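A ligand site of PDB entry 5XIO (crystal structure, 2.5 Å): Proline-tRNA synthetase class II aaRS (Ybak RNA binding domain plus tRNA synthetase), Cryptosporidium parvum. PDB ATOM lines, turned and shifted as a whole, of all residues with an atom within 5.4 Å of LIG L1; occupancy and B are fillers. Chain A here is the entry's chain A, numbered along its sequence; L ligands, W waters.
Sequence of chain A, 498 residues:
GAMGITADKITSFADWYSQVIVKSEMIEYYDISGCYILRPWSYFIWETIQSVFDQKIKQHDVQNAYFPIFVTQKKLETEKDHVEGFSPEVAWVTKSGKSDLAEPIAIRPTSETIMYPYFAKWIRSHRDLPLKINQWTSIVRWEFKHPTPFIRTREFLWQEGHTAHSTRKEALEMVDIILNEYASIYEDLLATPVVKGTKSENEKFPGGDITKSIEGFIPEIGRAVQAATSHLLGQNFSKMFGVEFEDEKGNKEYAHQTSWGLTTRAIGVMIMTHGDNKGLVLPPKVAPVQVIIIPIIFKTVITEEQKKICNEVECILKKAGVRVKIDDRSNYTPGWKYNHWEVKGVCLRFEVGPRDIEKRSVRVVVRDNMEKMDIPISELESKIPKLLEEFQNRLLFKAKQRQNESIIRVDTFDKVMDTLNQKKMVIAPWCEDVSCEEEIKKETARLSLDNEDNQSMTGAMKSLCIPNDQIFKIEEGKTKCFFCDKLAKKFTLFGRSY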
ATOM      1  N   ARG A 141      -8.751  16.499 -33.030  1.00  0.00           N
ATOM      2  CA  ARG A 141      -8.381  17.907 -32.715  1.00  0.00           C
ATOM      3  C   ARG A 141      -6.912  18.098 -32.841  1.00  0.00           C
ATOM      4  O   ARG A 141      -6.116  17.320 -32.321  1.00  0.00           O
ATOM      5  CB  ARG A 141      -8.787  18.295 -31.302  1.00  0.00           C
ATOM      6  CG  ARG A 141     -10.292  18.383 -31.104  1.00  0.00           C
ATOM      7  CD  ARG A 141     -10.629  18.601 -29.650  1.00  0.00           C
ATOM      8  NE  ARG A 141     -12.039  18.359 -29.357  1.00  0.00           N
ATOM      9  CZ  ARG A 141     -12.573  18.456 -28.130  1.00  0.00           C
ATOM     10  NH1 ARG A 141     -11.815  18.731 -27.085  1.00  0.00           N
ATOM     11  NH2 ARG A 141     -13.869  18.278 -27.933  1.00  0.00           N
ATOM     12  N   GLU A 143      -4.103  19.265 -31.602  1.00  0.00           N
ATOM     13  CA  GLU A 143      -3.532  19.807 -30.356  1.00  0.00           C
ATOM     14  C   GLU A 143      -2.216  20.601 -30.595  1.00  0.00           C
ATOM     15  O   GLU A 143      -1.347  20.152 -31.349  1.00  0.00           O
ATOM     16  CB  GLU A 143      -3.278  18.691 -29.319  1.00  0.00           C
ATOM     17  CG  GLU A 143      -4.532  17.987 -28.804  1.00  0.00           C
ATOM     18  CD  GLU A 143      -5.438  18.837 -27.890  1.00  0.00           C
ATOM     19  OE1 GLU A 143      -4.898  19.657 -27.068  1.00  0.00           O
ATOM     20  OE2 GLU A 143      -6.699  18.635 -27.963  1.00  0.00           O
ATOM     21  N   PHE A 150      -3.271   8.291 -24.081  1.00  0.00           N
ATOM     22  CA  PHE A 150      -4.561   8.522 -23.370  1.00  0.00           C
ATOM     23  C   PHE A 150      -4.941   9.935 -22.915  1.00  0.00           C
ATOM     24  O   PHE A 150      -6.005  10.460 -23.227  1.00  0.00           O
ATOM     25  CB  PHE A 150      -4.681   7.522 -22.185  1.00  0.00           C
ATOM     26  CG  PHE A 150      -4.538   6.070 -22.603  1.00  0.00           C
ATOM     27  CD1 PHE A 150      -5.531   5.459 -23.344  1.00  0.00           C
ATOM     28  CD2 PHE A 150      -3.420   5.337 -22.270  1.00  0.00           C
ATOM     29  CE1 PHE A 150      -5.434   4.115 -23.722  1.00  0.00           C
ATOM     30  CE2 PHE A 150      -3.275   4.032 -22.686  1.00  0.00           C
ATOM     31  CZ  PHE A 150      -4.283   3.424 -23.402  1.00  0.00           C
ATOM     32  N   ILE A 151      -4.095  10.560 -22.130  1.00  0.00           N
ATOM     33  CA  ILE A 151      -4.440  11.789 -21.540  1.00  0.00           C
ATOM     34  C   ILE A 151      -4.744  12.867 -22.589  1.00  0.00           C
ATOM     35  O   ILE A 151      -5.762  13.528 -22.465  1.00  0.00           O
ATOM     36  CB  ILE A 151      -3.308  12.270 -20.597  1.00  0.00           C
ATOM     37  CG1 ILE A 151      -2.904  11.211 -19.557  1.00  0.00           C
ATOM     38  CG2 ILE A 151      -3.695  13.537 -19.862  1.00  0.00           C
ATOM     39  CD1 ILE A 151      -3.803  11.001 -18.367  1.00  0.00           C
ATOM     40  N   ARG A 152      -3.838  13.040 -23.598  1.00  0.00           N
ATOM     41  CA  ARG A 152      -3.925  14.105 -24.641  1.00  0.00           C
ATOM     42  C   ARG A 152      -3.502  13.596 -26.028  1.00  0.00           C
ATOM     43  O   ARG A 152      -2.299  13.619 -26.381  1.00  0.00           O
ATOM     44  CB  ARG A 152      -3.043  15.330 -24.285  1.00  0.00           C
ATOM     45  CG  ARG A 152      -3.306  16.542 -25.203  1.00  0.00           C
ATOM     46  CD  ARG A 152      -2.466  17.791 -24.934  1.00  0.00           C
ATOM     47  NE  ARG A 152      -2.772  18.429 -23.668  1.00  0.00           N
ATOM     48  CZ  ARG A 152      -1.945  18.511 -22.642  1.00  0.00           C
ATOM     49  NH1 ARG A 152      -0.717  18.018 -22.743  1.00  0.00           N
ATOM     50  NH2 ARG A 152      -2.357  19.085 -21.523  1.00  0.00           N
ATOM     51  N   THR A 153      -4.483  13.129 -26.832  1.00  0.00           N
ATOM     52  CA  THR A 153      -4.230  12.617 -28.159  1.00  0.00           C
ATOM     53  C   THR A 153      -4.906  13.433 -29.267  1.00  0.00           C
ATOM     54  O   THR A 153      -5.857  14.193 -29.002  1.00  0.00           O
ATOM     55  CB  THR A 153      -4.683  11.160 -28.190  1.00  0.00           C
ATOM     56  OG1 THR A 153      -6.063  11.076 -27.897  1.00  0.00           O
ATOM     57  CG2 THR A 153      -3.966  10.317 -27.134  1.00  0.00           C
ATOM     58  N   ARG A 154      -4.409  13.318 -30.524  1.00  0.00           N
ATOM     59  CA  ARG A 154      -4.949  14.049 -31.682  1.00  0.00           C
ATOM     60  C   ARG A 154      -6.291  13.438 -32.088  1.00  0.00           C
ATOM     61  O   ARG A 154      -7.217  14.141 -32.385  1.00  0.00           O
ATOM     62  CB  ARG A 154      -4.065  13.946 -32.934  1.00  0.00           C
ATOM     63  CG  ARG A 154      -2.699  14.627 -32.931  1.00  0.00           C
ATOM     64  CD  ARG A 154      -2.773  16.121 -33.183  1.00  0.00           C
ATOM     65  NE  ARG A 154      -1.464  16.736 -33.028  1.00  0.00           N
ATOM     66  CZ  ARG A 154      -0.532  16.748 -33.984  1.00  0.00           C
ATOM     67  NH1 ARG A 154      -0.763  16.204 -35.192  1.00  0.00           N
ATOM     68  NH2 ARG A 154       0.625  17.316 -33.725  1.00  0.00           N
ATOM     69  N   PHE A 156      -8.982  10.833 -30.435  1.00  0.00           N
ATOM     70  CA  PHE A 156      -9.383  10.092 -29.241  1.00  0.00           C
ATOM     71  C   PHE A 156     -10.747   9.497 -29.412  1.00  0.00           C
ATOM     72  O   PHE A 156     -11.487   9.882 -30.368  1.00  0.00           O
ATOM     73  CB  PHE A 156      -9.311  10.935 -27.976  1.00  0.00           C
ATOM     74  CG  PHE A 156     -10.087  12.237 -28.009  1.00  0.00           C
ATOM     75  CD1 PHE A 156     -11.425  12.284 -27.722  1.00  0.00           C
ATOM     76  CD2 PHE A 156      -9.441  13.423 -28.214  1.00  0.00           C
ATOM     77  CE1 PHE A 156     -12.099  13.457 -27.662  1.00  0.00           C
ATOM     78  CE2 PHE A 156     -10.140  14.615 -28.216  1.00  0.00           C
ATOM     79  CZ  PHE A 156     -11.458  14.625 -27.956  1.00  0.00           C
ATOM     80  N   TRP A 158     -14.651   8.804 -27.666  1.00  0.00           N
ATOM     81  CA  TRP A 158     -15.531   9.280 -26.573  1.00  0.00           C
ATOM     82  C   TRP A 158     -16.998   8.918 -26.738  1.00  0.00           C
ATOM     83  O   TRP A 158     -17.405   8.332 -27.752  1.00  0.00           O
ATOM     84  CB  TRP A 158     -15.390  10.807 -26.420  1.00  0.00           C
ATOM     85  CG  TRP A 158     -16.194  11.714 -27.381  1.00  0.00           C
ATOM     86  CD1 TRP A 158     -16.913  11.377 -28.501  1.00  0.00           C
ATOM     87  CD2 TRP A 158     -16.300  13.149 -27.289  1.00  0.00           C
ATOM     88  NE1 TRP A 158     -17.428  12.515 -29.134  1.00  0.00           N
ATOM     89  CE2 TRP A 158     -17.081  13.605 -28.393  1.00  0.00           C
ATOM     90  CE3 TRP A 158     -15.773  14.083 -26.398  1.00  0.00           C
ATOM     91  CZ2 TRP A 158     -17.368  14.924 -28.610  1.00  0.00           C
ATOM     92  CZ3 TRP A 158     -16.055  15.391 -26.608  1.00  0.00           C
ATOM     93  CH2 TRP A 158     -16.870  15.823 -27.713  1.00  0.00           C
ATOM     94  N   GLN A 226      -8.604  17.086 -15.769  1.00  0.00           N
ATOM     95  CA  GLN A 226     -10.029  17.200 -15.836  1.00  0.00           C
ATOM     96  C   GLN A 226     -10.526  15.861 -16.396  1.00  0.00           C
ATOM     97  O   GLN A 226     -10.135  15.506 -17.499  1.00  0.00           O
ATOM     98  CB  GLN A 226     -10.453  18.358 -16.745  1.00  0.00           C
ATOM     99  CG  GLN A 226     -11.975  18.465 -16.787  1.00  0.00           C
ATOM    100  CD  GLN A 226     -12.549  19.538 -17.716  1.00  0.00           C
ATOM    101  OE1 GLN A 226     -13.222  20.451 -17.266  1.00  0.00           O
ATOM    102  NE2 GLN A 226     -12.348  19.398 -19.012  1.00  0.00           N
ATOM    103  N   ALA A 227     -11.387  15.137 -15.673  1.00  0.00           N
ATOM    104  CA  ALA A 227     -11.640  13.734 -16.001  1.00  0.00           C
ATOM    105  C   ALA A 227     -12.911  13.448 -16.773  1.00  0.00           C
ATOM    106  O   ALA A 227     -13.042  12.353 -17.348  1.00  0.00           O
ATOM    107  CB  ALA A 227     -11.590  12.853 -14.761  1.00  0.00           C
ATOM    108  N   ALA A 228     -13.853  14.382 -16.721  1.00  0.00           N
ATOM    109  CA  ALA A 228     -15.065  14.372 -17.524  1.00  0.00           C
ATOM    110  C   ALA A 228     -15.839  15.674 -17.239  1.00  0.00           C
ATOM    111  O   ALA A 228     -15.481  16.359 -16.316  1.00  0.00           O
ATOM    112  CB  ALA A 228     -15.889  13.174 -17.159  1.00  0.00           C
ATOM    113  N   THR A 229     -16.859  16.051 -18.019  1.00  0.00           N
ATOM    114  CA  THR A 229     -17.659  17.291 -17.757  1.00  0.00           C
ATOM    115  C   THR A 229     -19.092  17.210 -18.247  1.00  0.00           C
ATOM    116  O   THR A 229     -19.410  16.392 -19.126  1.00  0.00           O
ATOM    117  CB  THR A 229     -17.100  18.493 -18.520  1.00  0.00           C
ATOM    118  OG1 THR A 229     -16.539  18.013 -19.727  1.00  0.00           O
ATOM    119  CG2 THR A 229     -16.039  19.216 -17.738  1.00  0.00           C
ATOM    120  N   HIS A 231     -22.470  19.898 -18.928  1.00  0.00           N
ATOM    121  CA  HIS A 231     -22.933  21.294 -19.017  1.00  0.00           C
ATOM    122  C   HIS A 231     -24.490  21.452 -18.977  1.00  0.00           C
ATOM    123  O   HIS A 231     -25.265  20.679 -19.612  1.00  0.00           O
ATOM    124  CB  HIS A 231     -22.500  21.913 -20.342  1.00  0.00           C
ATOM    125  CG  HIS A 231     -21.088  21.664 -20.704  1.00  0.00           C
ATOM    126  ND1 HIS A 231     -20.039  22.317 -20.108  1.00  0.00           N
ATOM    127  CD2 HIS A 231     -20.533  20.831 -21.613  1.00  0.00           C
ATOM    128  CE1 HIS A 231     -18.910  21.907 -20.636  1.00  0.00           C
ATOM    129  NE2 HIS A 231     -19.176  21.016 -21.559  1.00  0.00           N
ATOM    130  N   GLY A 261     -19.561  14.733 -21.930  1.00  0.00           N
ATOM    131  CA  GLY A 261     -18.594  13.790 -22.605  1.00  0.00           C
ATOM    132  C   GLY A 261     -17.548  13.163 -21.688  1.00  0.00           C
ATOM    133  O   GLY A 261     -17.142  13.743 -20.682  1.00  0.00           O
ATOM    134  N   LEU A 262     -17.141  11.964 -22.033  1.00  0.00           N
ATOM    135  CA  LEU A 262     -16.018  11.243 -21.302  1.00  0.00           C
ATOM    136  C   LEU A 262     -15.174  10.460 -22.382  1.00  0.00           C
ATOM    137  O   LEU A 262     -15.780  10.018 -23.341  1.00  0.00           O
ATOM    138  CB  LEU A 262     -16.628  10.301 -20.231  1.00  0.00           C
ATOM    139  CG  LEU A 262     -15.615   9.447 -19.428  1.00  0.00           C
ATOM    140  CD1 LEU A 262     -16.216   8.967 -18.114  1.00  0.00           C
ATOM    141  CD2 LEU A 262     -15.154   8.248 -20.217  1.00  0.00           C
ATOM    142  N   THR A 263     -13.868  10.458 -22.225  1.00  0.00           N
ATOM    143  CA  THR A 263     -12.925   9.944 -23.200  1.00  0.00           C
ATOM    144  C   THR A 263     -11.967   8.909 -22.706  1.00  0.00           C
ATOM    145  O   THR A 263     -11.990   8.563 -21.581  1.00  0.00           O
ATOM    146  CB  THR A 263     -12.087  11.097 -23.839  1.00  0.00           C
ATOM    147  OG1 THR A 263     -11.095  11.547 -22.947  1.00  0.00           O
ATOM    148  CG2 THR A 263     -12.918  12.253 -24.208  1.00  0.00           C
ATOM    149  N   THR A 264     -11.196   8.363 -23.622  1.00  0.00           N
ATOM    150  CA  THR A 264     -10.099   7.379 -23.270  1.00  0.00           C
ATOM    151  C   THR A 264      -9.036   7.924 -22.338  1.00  0.00           C
ATOM    152  O   THR A 264      -8.110   7.195 -21.920  1.00  0.00           O
ATOM    153  CB  THR A 264      -9.380   6.906 -24.590  1.00  0.00           C
ATOM    154  OG1 THR A 264      -9.478   7.899 -25.639  1.00  0.00           O
ATOM    155  CG2 THR A 264     -10.040   5.702 -25.132  1.00  0.00           C
ATOM    156  N   ARG A 265      -9.071   9.246 -22.122  1.00  0.00           N
ATOM    157  CA  ARG A 265      -8.311   9.832 -21.010  1.00  0.00           C
ATOM    158  C   ARG A 265      -8.474   8.998 -19.701  1.00  0.00           C
ATOM    159  O   ARG A 265      -7.536   8.818 -18.940  1.00  0.00           O
ATOM    160  CB  ARG A 265      -8.786  11.237 -20.746  1.00  0.00           C
ATOM    161  CG  ARG A 265      -8.016  11.900 -19.606  1.00  0.00           C
ATOM    162  CD  ARG A 265      -8.411  13.350 -19.418  1.00  0.00           C
ATOM    163  NE  ARG A 265      -7.812  14.189 -20.446  1.00  0.00           N
ATOM    164  CZ  ARG A 265      -7.558  15.473 -20.320  1.00  0.00           C
ATOM    165  NH1 ARG A 265      -7.849  16.128 -19.223  1.00  0.00           N
ATOM    166  NH2 ARG A 265      -7.019  16.130 -21.311  1.00  0.00           N
HETATM  167  P1  LIG L   1      -9.398  20.204 -21.872  1.00  0.00           P
HETATM  168  O1  LIG L   1      -9.022  19.309 -20.800  1.00  0.00           O
HETATM  169  O2  LIG L   1      -8.569  21.513 -21.826  1.00  0.00           O
HETATM  170  O3  LIG L   1      -9.096  19.567 -23.240  1.00  0.00           O
HETATM  171  P2  LIG L   1     -11.746  20.847 -23.059  1.00  0.00           P
HETATM  172  O4  LIG L   1     -10.846  21.099 -24.268  1.00  0.00           O
HETATM  173  O5  LIG L   1     -12.771  21.842 -22.949  1.00  0.00           O
HETATM  174  N1  LIG L   1     -10.992  20.523 -21.694  1.00  0.00           N
HETATM  175  P3  LIG L   1     -14.038  19.106 -23.613  1.00  0.00           P
HETATM  176  O6  LIG L   1     -14.379  19.430 -24.970  1.00  0.00           O
HETATM  177  O7  LIG L   1     -14.849  19.666 -22.560  1.00  0.00           O
HETATM  178  O8  LIG L   1     -12.510  19.484 -23.370  1.00  0.00           O
HETATM  179  O9  LIG L   1     -14.010  17.535 -23.497  1.00  0.00           O
HETATM  180  C1  LIG L   1     -14.432  16.862 -22.325  1.00  0.00           C
HETATM  181  C2  LIG L   1     -13.425  15.795 -21.880  1.00  0.00           C
HETATM  182  O10 LIG L   1     -12.630  15.309 -22.962  1.00  0.00           O
HETATM  183  C3  LIG L   1     -12.432  16.545 -21.015  1.00  0.00           C
HETATM  184  O11 LIG L   1     -12.952  16.690 -19.674  1.00  0.00           O
HETATM  185  C4  LIG L   1     -11.192  15.677 -21.048  1.00  0.00           C
HETATM  186  O12 LIG L   1     -11.221  14.667 -20.025  1.00  0.00           O
HETATM  187  C5  LIG L   1     -11.319  14.990 -22.409  1.00  0.00           C
HETATM  188  N2  LIG L   1     -10.306  15.470 -23.382  1.00  0.00           N
HETATM  189  C6  LIG L   1     -10.201  16.726 -23.907  1.00  0.00           C
HETATM  190  N3  LIG L   1      -9.238  16.866 -24.813  1.00  0.00           N
HETATM  191  C7  LIG L   1      -8.725  15.583 -24.897  1.00  0.00           C
HETATM  192  C8  LIG L   1      -7.696  15.017 -25.669  1.00  0.00           C
HETATM  193  N4  LIG L   1      -6.970  15.741 -26.519  1.00  0.00           N
HETATM  194  N5  LIG L   1      -7.405  13.724 -25.537  1.00  0.00           N
HETATM  195  C9  LIG L   1      -8.109  12.998 -24.690  1.00  0.00           C
HETATM  196  N6  LIG L   1      -9.098  13.418 -23.903  1.00  0.00           N
HETATM  197  C10 LIG L   1      -9.385  14.718 -24.041  1.00  0.00           C
HETATM  198  O1  LG2 L   2     -16.662  19.986 -26.842  1.00  0.00           O
HETATM  199  C1  LG2 L   2     -16.967  20.934 -26.158  1.00  0.00           C
HETATM  200  C2  LG2 L   2     -18.279  21.019 -25.395  1.00  0.00           C
HETATM  201  C3  LG2 L   2     -18.934  19.638 -25.216  1.00  0.00           C
HETATM  202  N1  LG2 L   2     -19.437  19.097 -26.463  1.00  0.00           N
HETATM  203  C4  LG2 L   2     -20.211  17.887 -26.227  1.00  0.00           C
HETATM  204  C5  LG2 L   2     -19.404  16.837 -25.488  1.00  0.00           C
HETATM  205  C6  LG2 L   2     -18.800  17.408 -24.220  1.00  0.00           C
HETATM  206  C7  LG2 L   2     -18.007  18.653 -24.537  1.00  0.00           C
HETATM  207  O2  LG2 L   2     -17.493  19.197 -23.346  1.00  0.00           O
HETATM  208  C8  LG2 L   2     -16.061  22.156 -26.021  1.00  0.00           C
HETATM  209  N2  LG2 L   2     -15.077  22.180 -27.111  1.00  0.00           N
HETATM  210  C9  LG2 L   2     -15.438  22.751 -28.320  1.00  0.00           C
HETATM  211  O3  LG2 L   2     -16.547  23.178 -28.510  1.00  0.00           O
HETATM  212  C10 LG2 L   2     -14.396  22.709 -29.344  1.00  0.00           C
HETATM  213  C11 LG2 L   2     -14.638  23.226 -30.613  1.00  0.00           C
HETATM  214  C12 LG2 L   2     -13.836  21.702 -26.920  1.00  0.00           C
HETATM  215  N3  LG2 L   2     -12.900  21.661 -27.784  1.00  0.00           N
HETATM  216  C13 LG2 L   2     -13.159  22.169 -29.042  1.00  0.00           C
HETATM  217  C14 LG2 L   2     -12.167  22.140 -30.002  1.00  0.00           C
HETATM  218  C15 LG2 L   2     -12.379  22.645 -31.280  1.00  0.00           C
HETATM  219 BR1  LG2 L   2     -10.982  22.532 -32.548  1.00  0.00          BR
HETATM  220  C16 LG2 L   2     -13.639  23.187 -31.579  1.00  0.00           C
HETATM  221 CL1  LG2 L   2     -13.961  23.835 -33.124  1.00  0.00          CL
HETATM  222  O   HOH W   1      -8.188  24.061 -21.484  1.00  0.00           O
HETATM  223  O   HOH W   2     -12.857  12.266 -20.225  1.00  0.00           O
HETATM  224  O   HOH W   3      -8.980  18.991 -26.749  1.00  0.00           O
HETATM  225  O   HOH W   4     -14.898  23.694 -22.721  1.00  0.00           O
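Water W3 lies within hydrogen-bond range of OE2 of Glu 143 (2.6 Å), NH1 of Arg 141 (2.9 Å) and N3 of LIG L1 (2.9 Å).
Water W2 lies within hydrogen-bond range of N of Thr 263 (2.9 Å), O of Ala 227 (2.9 Å) and O12 of LIG L1 (2.9 Å).
The backbone NH of Thr 153 is in hydrogen-bond range of a nitrogen (N5) of LIG L1 (3.3 Å).
O of Thr 153 sits at hydrogen-bond distance from N4 of LIG L1.
A ring nitrogen (NE2) of His 231 is in hydrogen-bond range of an oxygen (O2) of LG2 L2 (3.1 Å).
NH1 of Arg 141 is in hydrogen-bond range of N3 of LG2 L2 (3.2 Å).
OE2 of Glu 143 sits at hydrogen-bond distance from N4 of LIG L1, 3.2 Å away.
An oxygen (O1) of LIG L1 lies within salt-bridge range of the guanidinium group of Arg 265.
The backbone carbonyl oxygen (O) of Gln 226 sits at hydrogen-bond distance from an oxygen (O12) of LIG L1.
A nitrogen (N6) of LIG L1 lies within hydrogen-bond range of the side-chain hydroxyl of Thr 263 (2.9 Å).
An oxygen (O6) of LIG L1 lies within salt-bridge range of the guanidinium group of Arg 141.
NE2 of Gln 226 sits at hydrogen-bond distance from O11 of LIG L1, 2.9 Å away.
O7 of LIG L1 sits at hydrogen-bond distance from O2 of LG2 L2, 2.8 Å away.
OG1 of Thr 263 lies close to N of Arg 265 (3.2 Å).
The guanidinium group (NE) of Arg 265 is in hydrogen-bond range of the backbone carbonyl oxygen (O) of Ile 151 (3.0 Å).
The backbone NH (N) of Arg 265 sits close to the backbone carbonyl oxygen (O) of Phe 150 (3.5 Å).
The backbone carbonyl oxygen of Gln 226 sits at hydrogen-bond distance from the guanidinium group of Arg 265 (2.9 Å).
The backbone carbonyl oxygen (O) of Thr 229 is in hydrogen-bond range of the backbone NH (N) of Gly 261, 3.3 Å away.
N of Arg 141 is in hydrogen-bond range of O of Arg 154 (2.9 Å).
The backbone carbonyl oxygen (O) of Ile 151 sits close to a nitrogen (N5) of LIG L1 (3.5 Å).
Merely in contact with LIG L1: Phe 156, Thr 229, Phe 150, Arg 152, Ala 228 and Ala 227.
Hydrophobic or aromatic side chains within 4 Å of LIG L1: Phe 156.
The nearest printed residue that does not touch LIG L1 is Trp 158 (4.3 Å).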
